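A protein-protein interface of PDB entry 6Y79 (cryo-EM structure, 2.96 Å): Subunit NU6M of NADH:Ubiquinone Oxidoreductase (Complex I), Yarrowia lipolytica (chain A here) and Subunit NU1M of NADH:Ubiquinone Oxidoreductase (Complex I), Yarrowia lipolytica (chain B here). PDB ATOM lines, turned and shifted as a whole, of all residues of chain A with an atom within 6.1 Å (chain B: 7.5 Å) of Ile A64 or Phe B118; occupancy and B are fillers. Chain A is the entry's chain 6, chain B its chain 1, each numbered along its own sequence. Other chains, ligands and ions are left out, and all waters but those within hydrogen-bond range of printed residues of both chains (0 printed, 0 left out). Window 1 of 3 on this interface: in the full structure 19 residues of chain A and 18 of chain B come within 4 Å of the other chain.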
ATOM      1  N   LEU A  34       5.694  27.940   3.130  1.00  0.00           N
ATOM      2  CA  LEU A  34       4.415  27.740   2.464  1.00  0.00           C
ATOM      3  C   LEU A  34       3.417  28.789   2.903  1.00  0.00           C
ATOM      4  O   LEU A  34       2.547  29.196   2.121  1.00  0.00           O
ATOM      5  CB  LEU A  34       3.881  26.352   2.752  1.00  0.00           C
ATOM      6  CG  LEU A  34       4.750  25.242   2.204  1.00  0.00           C
ATOM      7  CD1 LEU A  34       4.206  23.936   2.684  1.00  0.00           C
ATOM      8  CD2 LEU A  34       4.852  25.323   0.707  1.00  0.00           C
ATOM      9  N   ILE A  37       4.090  31.629   0.579  1.00  0.00           N
ATOM     10  CA  ILE A  37       3.424  31.427  -0.717  1.00  0.00           C
ATOM     11  C   ILE A  37       1.933  31.757  -0.622  1.00  0.00           C
ATOM     12  O   ILE A  37       1.347  32.381  -1.526  1.00  0.00           O
ATOM     13  CB  ILE A  37       3.654  29.985  -1.210  1.00  0.00           C
ATOM     14  CG1 ILE A  37       5.139  29.729  -1.430  1.00  0.00           C
ATOM     15  CG2 ILE A  37       2.892  29.700  -2.492  1.00  0.00           C
ATOM     16  CD1 ILE A  37       5.442  28.321  -1.861  1.00  0.00           C
ATOM     17  N   PHE A  40       1.597  35.490  -0.767  1.00  0.00           N
ATOM     18  CA  PHE A  40       1.635  35.936  -2.163  1.00  0.00           C
ATOM     19  C   PHE A  40       0.275  35.784  -2.834  1.00  0.00           C
ATOM     20  O   PHE A  40      -0.145  36.648  -3.615  1.00  0.00           O
ATOM     21  CB  PHE A  40       2.670  35.143  -2.960  1.00  0.00           C
ATOM     22  CG  PHE A  40       4.093  35.489  -2.652  1.00  0.00           C
ATOM     23  CD1 PHE A  40       4.582  36.752  -2.898  1.00  0.00           C
ATOM     24  CD2 PHE A  40       4.962  34.526  -2.178  1.00  0.00           C
ATOM     25  CE1 PHE A  40       5.894  37.075  -2.610  1.00  0.00           C
ATOM     26  CE2 PHE A  40       6.275  34.832  -1.905  1.00  0.00           C
ATOM     27  CZ  PHE A  40       6.744  36.108  -2.120  1.00  0.00           C
ATOM     28  N   VAL A  41      -0.424  34.682  -2.542  1.00  0.00           N
ATOM     29  CA  VAL A  41      -1.754  34.467  -3.117  1.00  0.00           C
ATOM     30  C   VAL A  41      -2.766  35.479  -2.570  1.00  0.00           C
ATOM     31  O   VAL A  41      -3.611  35.991  -3.315  1.00  0.00           O
ATOM     32  CB  VAL A  41      -2.195  33.012  -2.875  1.00  0.00           C
ATOM     33  CG1 VAL A  41      -3.613  32.776  -3.334  1.00  0.00           C
ATOM     34  CG2 VAL A  41      -1.271  32.070  -3.599  1.00  0.00           C
ATOM     35  N   TYR A  59       2.453  38.452 -10.279  1.00  0.00           N
ATOM     36  CA  TYR A  59       2.919  38.030  -8.956  1.00  0.00           C
ATOM     37  C   TYR A  59       2.964  36.517  -8.848  1.00  0.00           C
ATOM     38  O   TYR A  59       3.895  35.953  -8.267  1.00  0.00           O
ATOM     39  CB  TYR A  59       2.010  38.567  -7.846  1.00  0.00           C
ATOM     40  CG  TYR A  59       2.170  40.024  -7.493  1.00  0.00           C
ATOM     41  CD1 TYR A  59       3.316  40.495  -6.888  1.00  0.00           C
ATOM     42  CD2 TYR A  59       1.138  40.911  -7.690  1.00  0.00           C
ATOM     43  CE1 TYR A  59       3.454  41.827  -6.559  1.00  0.00           C
ATOM     44  CE2 TYR A  59       1.269  42.229  -7.392  1.00  0.00           C
ATOM     45  CZ  TYR A  59       2.414  42.688  -6.811  1.00  0.00           C
ATOM     46  OH  TYR A  59       2.494  44.019  -6.495  1.00  0.00           O
ATOM     47  N   ILE A  60       1.926  35.848  -9.351  1.00  0.00           N
ATOM     48  CA  ILE A  60       1.880  34.391  -9.314  1.00  0.00           C
ATOM     49  C   ILE A  60       2.963  33.796 -10.208  1.00  0.00           C
ATOM     50  O   ILE A  60       3.566  32.772  -9.868  1.00  0.00           O
ATOM     51  CB  ILE A  60       0.462  33.921  -9.693  1.00  0.00           C
ATOM     52  CG1 ILE A  60      -0.523  34.339  -8.609  1.00  0.00           C
ATOM     53  CG2 ILE A  60       0.381  32.419  -9.864  1.00  0.00           C
ATOM     54  CD1 ILE A  60      -1.955  34.165  -9.001  1.00  0.00           C
ATOM     55  N   MET A  61       3.282  34.453 -11.319  1.00  0.00           N
ATOM     56  CA  MET A  61       4.305  33.918 -12.206  1.00  0.00           C
ATOM     57  C   MET A  61       5.705  34.148 -11.653  1.00  0.00           C
ATOM     58  O   MET A  61       6.518  33.222 -11.598  1.00  0.00           O
ATOM     59  CB  MET A  61       4.163  34.541 -13.587  1.00  0.00           C
ATOM     60  CG  MET A  61       5.259  34.159 -14.544  1.00  0.00           C
ATOM     61  SD  MET A  61       4.984  34.888 -16.159  1.00  0.00           S
ATOM     62  CE  MET A  61       3.235  34.574 -16.333  1.00  0.00           C
ATOM     63  N   ILE A  62       6.008  35.372 -11.235  1.00  0.00           N
ATOM     64  CA  ILE A  62       7.376  35.718 -10.869  1.00  0.00           C
ATOM     65  C   ILE A  62       7.682  35.369  -9.419  1.00  0.00           C
ATOM     66  O   ILE A  62       8.670  34.693  -9.134  1.00  0.00           O
ATOM     67  CB  ILE A  62       7.634  37.208 -11.171  1.00  0.00           C
ATOM     68  CG1 ILE A  62       7.723  37.420 -12.682  1.00  0.00           C
ATOM     69  CG2 ILE A  62       8.906  37.687 -10.499  1.00  0.00           C
ATOM     70  CD1 ILE A  62       7.582  38.856 -13.108  1.00  0.00           C
ATOM     71  N   TYR A  63       6.853  35.809  -8.472  1.00  0.00           N
ATOM     72  CA  TYR A  63       7.179  35.603  -7.063  1.00  0.00           C
ATOM     73  C   TYR A  63       6.953  34.162  -6.637  1.00  0.00           C
ATOM     74  O   TYR A  63       7.812  33.559  -5.987  1.00  0.00           O
ATOM     75  CB  TYR A  63       6.358  36.535  -6.180  1.00  0.00           C
ATOM     76  CG  TYR A  63       6.781  37.975  -6.236  1.00  0.00           C
ATOM     77  CD1 TYR A  63       6.290  38.817  -7.217  1.00  0.00           C
ATOM     78  CD2 TYR A  63       7.680  38.492  -5.316  1.00  0.00           C
ATOM     79  CE1 TYR A  63       6.674  40.136  -7.280  1.00  0.00           C
ATOM     80  CE2 TYR A  63       8.064  39.815  -5.366  1.00  0.00           C
ATOM     81  CZ  TYR A  63       7.555  40.630  -6.350  1.00  0.00           C
ATOM     82  OH  TYR A  63       7.933  41.948  -6.408  1.00  0.00           O
ATOM     83  N   ILE A  64       5.798  33.598  -6.978  1.00  0.00           N
ATOM     84  CA  ILE A  64       5.510  32.225  -6.587  1.00  0.00           C
ATOM     85  C   ILE A  64       6.313  31.252  -7.437  1.00  0.00           C
ATOM     86  O   ILE A  64       6.998  30.369  -6.916  1.00  0.00           O
ATOM     87  CB  ILE A  64       4.003  31.945  -6.682  1.00  0.00           C
ATOM     88  CG1 ILE A  64       3.234  32.849  -5.728  1.00  0.00           C
ATOM     89  CG2 ILE A  64       3.726  30.528  -6.325  1.00  0.00           C
ATOM     90  CD1 ILE A  64       1.747  32.635  -5.742  1.00  0.00           C
ATOM     91  N   GLY A  65       6.275  31.423  -8.753  1.00  0.00           N
ATOM     92  CA  GLY A  65       6.862  30.456  -9.654  1.00  0.00           C
ATOM     93  C   GLY A  65       8.360  30.492  -9.820  1.00  0.00           C
ATOM     94  O   GLY A  65       8.917  29.567 -10.412  1.00  0.00           O
ATOM     95  N   ALA A  66       9.038  31.542  -9.368  1.00  0.00           N
ATOM     96  CA  ALA A  66      10.491  31.592  -9.454  1.00  0.00           C
ATOM     97  C   ALA A  66      11.159  31.804  -8.107  1.00  0.00           C
ATOM     98  O   ALA A  66      12.092  31.072  -7.766  1.00  0.00           O
ATOM     99  CB  ALA A  66      10.928  32.690 -10.432  1.00  0.00           C
ATOM    100  N   ILE A  67      10.707  32.786  -7.327  1.00  0.00           N
ATOM    101  CA  ILE A  67      11.391  33.126  -6.084  1.00  0.00           C
ATOM    102  C   ILE A  67      11.092  32.091  -5.007  1.00  0.00           C
ATOM    103  O   ILE A  67      11.999  31.635  -4.296  1.00  0.00           O
ATOM    104  CB  ILE A  67      11.003  34.551  -5.648  1.00  0.00           C
ATOM    105  CG1 ILE A  67      11.519  35.571  -6.661  1.00  0.00           C
ATOM    106  CG2 ILE A  67      11.549  34.878  -4.283  1.00  0.00           C
ATOM    107  CD1 ILE A  67      10.948  36.948  -6.474  1.00  0.00           C
ATOM    108  N   ALA A  68       9.830  31.674  -4.892  1.00  0.00           N
ATOM    109  CA  ALA A  68       9.473  30.661  -3.907  1.00  0.00           C
ATOM    110  C   ALA A  68      10.019  29.294  -4.292  1.00  0.00           C
ATOM    111  O   ALA A  68      10.386  28.504  -3.421  1.00  0.00           O
ATOM    112  CB  ALA A  68       7.960  30.601  -3.736  1.00  0.00           C
ATOM    113  N   VAL A  69      10.114  29.013  -5.589  1.00  0.00           N
ATOM    114  CA  VAL A  69      10.692  27.751  -6.045  1.00  0.00           C
ATOM    115  C   VAL A  69      12.181  27.699  -5.734  1.00  0.00           C
ATOM    116  O   VAL A  69      12.697  26.673  -5.275  1.00  0.00           O
ATOM    117  CB  VAL A  69      10.415  27.568  -7.544  1.00  0.00           C
ATOM    118  CG1 VAL A  69      11.004  26.279  -8.050  1.00  0.00           C
ATOM    119  CG2 VAL A  69       8.940  27.593  -7.772  1.00  0.00           C
ATOM    120  N   LEU A  72      12.403  27.194  -1.788  1.00  0.00           N
ATOM    121  CA  LEU A  72      12.148  25.803  -1.397  1.00  0.00           C
ATOM    122  C   LEU A  72      13.278  24.886  -1.842  1.00  0.00           C
ATOM    123  O   LEU A  72      13.676  23.964  -1.112  1.00  0.00           O
ATOM    124  CB  LEU A  72      10.837  25.305  -2.007  1.00  0.00           C
ATOM    125  CG  LEU A  72       9.472  25.282  -1.325  1.00  0.00           C
ATOM    126  CD1 LEU A  72       8.823  26.610  -1.376  1.00  0.00           C
ATOM    127  CD2 LEU A  72       8.594  24.314  -2.044  1.00  0.00           C
ATOM    128  N   SER B  76      -0.075  17.819  -1.158  1.00  0.00           N
ATOM    129  CA  SER B  76       0.646  17.999  -2.426  1.00  0.00           C
ATOM    130  C   SER B  76      -0.034  17.296  -3.616  1.00  0.00           C
ATOM    131  O   SER B  76      -0.033  17.893  -4.713  1.00  0.00           O
ATOM    132  CB  SER B  76       2.144  17.624  -2.294  1.00  0.00           C
ATOM    133  OG  SER B  76       2.449  16.283  -1.935  1.00  0.00           O
ATOM    134  N   ILE B  79      -2.850  19.979  -4.498  1.00  0.00           N
ATOM    135  CA  ILE B  79      -2.446  21.231  -5.137  1.00  0.00           C
ATOM    136  C   ILE B  79      -1.924  20.963  -6.547  1.00  0.00           C
ATOM    137  O   ILE B  79      -2.194  21.755  -7.470  1.00  0.00           O
ATOM    138  CB  ILE B  79      -1.453  21.997  -4.245  1.00  0.00           C
ATOM    139  CG1 ILE B  79      -2.111  22.343  -2.905  1.00  0.00           C
ATOM    140  CG2 ILE B  79      -1.030  23.332  -4.860  1.00  0.00           C
ATOM    141  CD1 ILE B  79      -3.392  23.160  -3.031  1.00  0.00           C
ATOM    142  N   THR B  80      -1.330  19.785  -6.787  1.00  0.00           N
ATOM    143  CA  THR B  80      -1.012  19.445  -8.176  1.00  0.00           C
ATOM    144  C   THR B  80      -2.259  19.021  -8.963  1.00  0.00           C
ATOM    145  O   THR B  80      -2.379  19.374 -10.139  1.00  0.00           O
ATOM    146  CB  THR B  80       0.097  18.390  -8.219  1.00  0.00           C
ATOM    147  OG1 THR B  80       1.277  18.997  -7.711  1.00  0.00           O
ATOM    148  CG2 THR B  80       0.438  17.962  -9.625  1.00  0.00           C
ATOM    149  N   THR B  83      -4.168  22.531  -9.700  1.00  0.00           N
ATOM    150  CA  THR B  83      -3.606  23.416 -10.731  1.00  0.00           C
ATOM    151  C   THR B  83      -3.317  22.684 -12.044  1.00  0.00           C
ATOM    152  O   THR B  83      -3.145  23.327 -13.085  1.00  0.00           O
ATOM    153  CB  THR B  83      -2.366  24.146 -10.228  1.00  0.00           C
ATOM    154  OG1 THR B  83      -1.347  23.227  -9.864  1.00  0.00           O
ATOM    155  CG2 THR B  83      -2.723  25.041  -9.061  1.00  0.00           C
ATOM    156  N   ALA B 111       0.744  31.375 -15.911  1.00  0.00           N
ATOM    157  CA  ALA B 111       0.900  31.444 -14.467  1.00  0.00           C
ATOM    158  C   ALA B 111       0.481  30.153 -13.780  1.00  0.00           C
ATOM    159  O   ALA B 111       1.045  29.809 -12.738  1.00  0.00           O
ATOM    160  CB  ALA B 111       0.094  32.613 -13.909  1.00  0.00           C
ATOM    161  N   SER B 114       3.263  27.444 -14.093  1.00  0.00           N
ATOM    162  CA  SER B 114       4.379  27.599 -13.177  1.00  0.00           C
ATOM    163  C   SER B 114       4.027  27.167 -11.763  1.00  0.00           C
ATOM    164  O   SER B 114       4.931  26.951 -10.952  1.00  0.00           O
ATOM    165  CB  SER B 114       4.847  29.049 -13.164  1.00  0.00           C
ATOM    166  OG  SER B 114       3.879  29.868 -12.535  1.00  0.00           O
ATOM    167  N   LEU B 115       2.737  27.050 -11.446  1.00  0.00           N
ATOM    168  CA  LEU B 115       2.303  26.540 -10.153  1.00  0.00           C
ATOM    169  C   LEU B 115       2.432  25.031 -10.044  1.00  0.00           C
ATOM    170  O   LEU B 115       2.325  24.497  -8.937  1.00  0.00           O
ATOM    171  CB  LEU B 115       0.850  26.926  -9.883  1.00  0.00           C
ATOM    172  CG  LEU B 115       0.502  28.398  -9.720  1.00  0.00           C
ATOM    173  CD1 LEU B 115      -0.987  28.559  -9.569  1.00  0.00           C
ATOM    174  CD2 LEU B 115       1.200  28.956  -8.520  1.00  0.00           C
ATOM    175  N   GLY B 116       2.655  24.338 -11.153  1.00  0.00           N
ATOM    176  CA  GLY B 116       2.712  22.897 -11.151  1.00  0.00           C
ATOM    177  C   GLY B 116       4.027  22.297 -10.742  1.00  0.00           C
ATOM    178  O   GLY B 116       4.137  21.071 -10.662  1.00  0.00           O
ATOM    179  N   VAL B 117       5.038  23.123 -10.476  1.00  0.00           N
ATOM    180  CA  VAL B 117       6.329  22.592 -10.064  1.00  0.00           C
ATOM    181  C   VAL B 117       6.320  22.138  -8.608  1.00  0.00           C
ATOM    182  O   VAL B 117       7.033  21.179  -8.269  1.00  0.00           O
ATOM    183  CB  VAL B 117       7.434  23.632 -10.324  1.00  0.00           C
ATOM    184  CG1 VAL B 117       7.502  23.965 -11.802  1.00  0.00           C
ATOM    185  CG2 VAL B 117       7.181  24.901  -9.555  1.00  0.00           C
ATOM    186  N   PHE B 118       5.463  22.749  -7.774  1.00  0.00           N
ATOM    187  CA  PHE B 118       5.560  22.618  -6.324  1.00  0.00           C
ATOM    188  C   PHE B 118       5.309  21.195  -5.880  1.00  0.00           C
ATOM    189  O   PHE B 118       6.147  20.612  -5.191  1.00  0.00           O
ATOM    190  CB  PHE B 118       4.586  23.569  -5.644  1.00  0.00           C
ATOM    191  CG  PHE B 118       4.981  24.991  -5.770  1.00  0.00           C
ATOM    192  CD1 PHE B 118       5.941  25.525  -4.932  1.00  0.00           C
ATOM    193  CD2 PHE B 118       4.428  25.785  -6.752  1.00  0.00           C
ATOM    194  CE1 PHE B 118       6.324  26.827  -5.059  1.00  0.00           C
ATOM    195  CE2 PHE B 118       4.807  27.089  -6.881  1.00  0.00           C
ATOM    196  CZ  PHE B 118       5.756  27.607  -6.032  1.00  0.00           C
ATOM    197  N   GLY B 119       4.242  20.578  -6.380  1.00  0.00           N
ATOM    198  CA  GLY B 119       3.920  19.208  -6.035  1.00  0.00           C
ATOM    199  C   GLY B 119       4.941  18.173  -6.454  1.00  0.00           C
ATOM    200  O   GLY B 119       4.823  17.023  -6.023  1.00  0.00           O
ATOM    201  N   SER B 120       5.937  18.536  -7.264  1.00  0.00           N
ATOM    202  CA  SER B 120       7.104  17.670  -7.277  1.00  0.00           C
ATOM    203  C   SER B 120       8.001  17.965  -6.079  1.00  0.00           C
ATOM    204  O   SER B 120       8.131  17.125  -5.180  1.00  0.00           O
ATOM    205  CB  SER B 120       7.883  17.837  -8.578  1.00  0.00           C
ATOM    206  OG  SER B 120       9.059  17.053  -8.543  1.00  0.00           O
ATOM    207  N   LEU B 121       8.529  19.197  -6.037  1.00  0.00           N
ATOM    208  CA  LEU B 121       9.532  19.625  -5.063  1.00  0.00           C
ATOM    209  C   LEU B 121       9.049  19.457  -3.631  1.00  0.00           C
ATOM    210  O   LEU B 121       9.746  18.858  -2.800  1.00  0.00           O
ATOM    211  CB  LEU B 121       9.887  21.088  -5.318  1.00  0.00           C
ATOM    212  CG  LEU B 121      11.042  21.721  -4.557  1.00  0.00           C
ATOM    213  CD1 LEU B 121      12.322  20.948  -4.801  1.00  0.00           C
ATOM    214  CD2 LEU B 121      11.186  23.148  -5.015  1.00  0.00           C
ATOM    215  N   LEU B 122       7.845  19.964  -3.346  1.00  0.00           N
ATOM    216  CA  LEU B 122       7.219  19.849  -2.033  1.00  0.00           C
ATOM    217  C   LEU B 122       7.079  18.397  -1.605  1.00  0.00           C
ATOM    218  O   LEU B 122       7.379  18.054  -0.456  1.00  0.00           O
ATOM    219  CB  LEU B 122       5.864  20.549  -2.077  1.00  0.00           C
ATOM    220  CG  LEU B 122       4.753  20.631  -1.061  1.00  0.00           C
ATOM    221  CD1 LEU B 122       5.098  21.712  -0.120  1.00  0.00           C
ATOM    222  CD2 LEU B 122       3.490  20.999  -1.821  1.00  0.00           C
ATOM    223  N   SER B 123       6.718  17.510  -2.532  1.00  0.00           N
ATOM    224  CA  SER B 123       6.534  16.121  -2.136  1.00  0.00           C
ATOM    225  C   SER B 123       7.849  15.363  -2.069  1.00  0.00           C
ATOM    226  O   SER B 123       7.854  14.182  -1.719  1.00  0.00           O
ATOM    227  CB  SER B 123       5.568  15.416  -3.086  1.00  0.00           C
ATOM    228  OG  SER B 123       6.126  15.302  -4.378  1.00  0.00           O
ATOM    229  N   GLY B 124       8.961  15.999  -2.419  1.00  0.00           N
ATOM    230  CA  GLY B 124      10.241  15.452  -2.023  1.00  0.00           C
ATOM    231  C   GLY B 124      10.481  15.607  -0.540  1.00  0.00           C
ATOM    232  O   GLY B 124      11.140  14.762   0.080  1.00  0.00           O
ATOM    233  N   THR B 140      12.679  18.809 -10.132  1.00  0.00           N
ATOM    234  CA  THR B 140      12.252  20.202 -10.200  1.00  0.00           C
ATOM    235  C   THR B 140      13.215  21.043 -11.035  1.00  0.00           C
ATOM    236  O   THR B 140      12.788  21.981 -11.719  1.00  0.00           O
ATOM    237  CB  THR B 140      12.094  20.740  -8.779  1.00  0.00           C
ATOM    238  OG1 THR B 140      11.137  19.925  -8.100  1.00  0.00           O
ATOM    239  CG2 THR B 140      11.583  22.173  -8.761  1.00  0.00           C
ATOM    240  N   LEU B 143      12.171  20.452 -14.509  1.00  0.00           N
ATOM    241  CA  LEU B 143      10.848  21.050 -14.673  1.00  0.00           C
ATOM    242  C   LEU B 143      10.929  22.550 -14.948  1.00  0.00           C
ATOM    243  O   LEU B 143      10.351  23.051 -15.929  1.00  0.00           O
ATOM    244  CB  LEU B 143      10.047  20.771 -13.405  1.00  0.00           C
ATOM    245  CG  LEU B 143       8.531  20.756 -13.343  1.00  0.00           C
ATOM    246  CD1 LEU B 143       8.001  20.076 -14.543  1.00  0.00           C
ATOM    247  CD2 LEU B 143       8.109  20.000 -12.101  1.00  0.00           C
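Of chain B, only Leu B115 and Phe B118 come within 4 Å of Ile A64. Of chain A, only Ile A37, Ile A64 and Val A69 come within 4 Å of Phe B118. Of the printed residues of chain A, Ala B111 touches Ile A60. Of the printed residues of chain A, Ser B114 touches Ile A60.
The backbone NH (N) of Gly A65 sits at hydrogen-bond distance from the backbone carbonyl oxygen (O) of Ile A60 (3.2 Å). The side-chain hydroxyl (OG) of Ser B114 lies within hydrogen-bond range of the backbone carbonyl oxygen (O) of Ala B111 (2.8 Å). The backbone NH (N) of Leu B121 sits close to the side-chain hydroxyl (OG1) of Thr B140 (3.4 Å). O of Tyr A59 is in hydrogen-bond range of N of Ile A64.
Among the printed residues, merely in contact across the chains: Ile A64 with Phe B118 (3.2 Å), Val A69 with Phe B118 (3.6 Å), Ile A37 with Phe B118 (3.6 Å), Val A69 with Val B117 (3.7 Å), Leu A34 with Leu B122 (3.7 Å), Ile A64 with Leu B115 (3.7 Å), Leu A72 with Leu B121 (3.7 Å), Ile A60 with Leu B115 (3.8 Å), Val A69 with Leu B121 (3.8 Å), Ile A60 with Ala B111 (3.9 Å) and Ile A60 with Ser B114 (3.96 Å).
Printed residues of chain A that touch a printed residue of chain B: Leu A34, Ile A37, Ile A60, Ile A64, Val A69 and Leu A72. Printed residues of chain B that touch a printed residue of chain A: Ala B111, Ser B114, Leu B115, Val B117, Phe B118, Leu B121 and Leu B122. Hydrophobic or aromatic side chains of chain B within 4 Å of the printed part of chain A: Leu B115, Val B117, Phe B118, Leu B121 and Leu B122. Among the printed residues, 11 pairs touch across the chains. Among the printed residues, no Asp or Glu carboxylate lies within 4 Å of a Lys or Arg side-chain nitrogen of the other chain.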
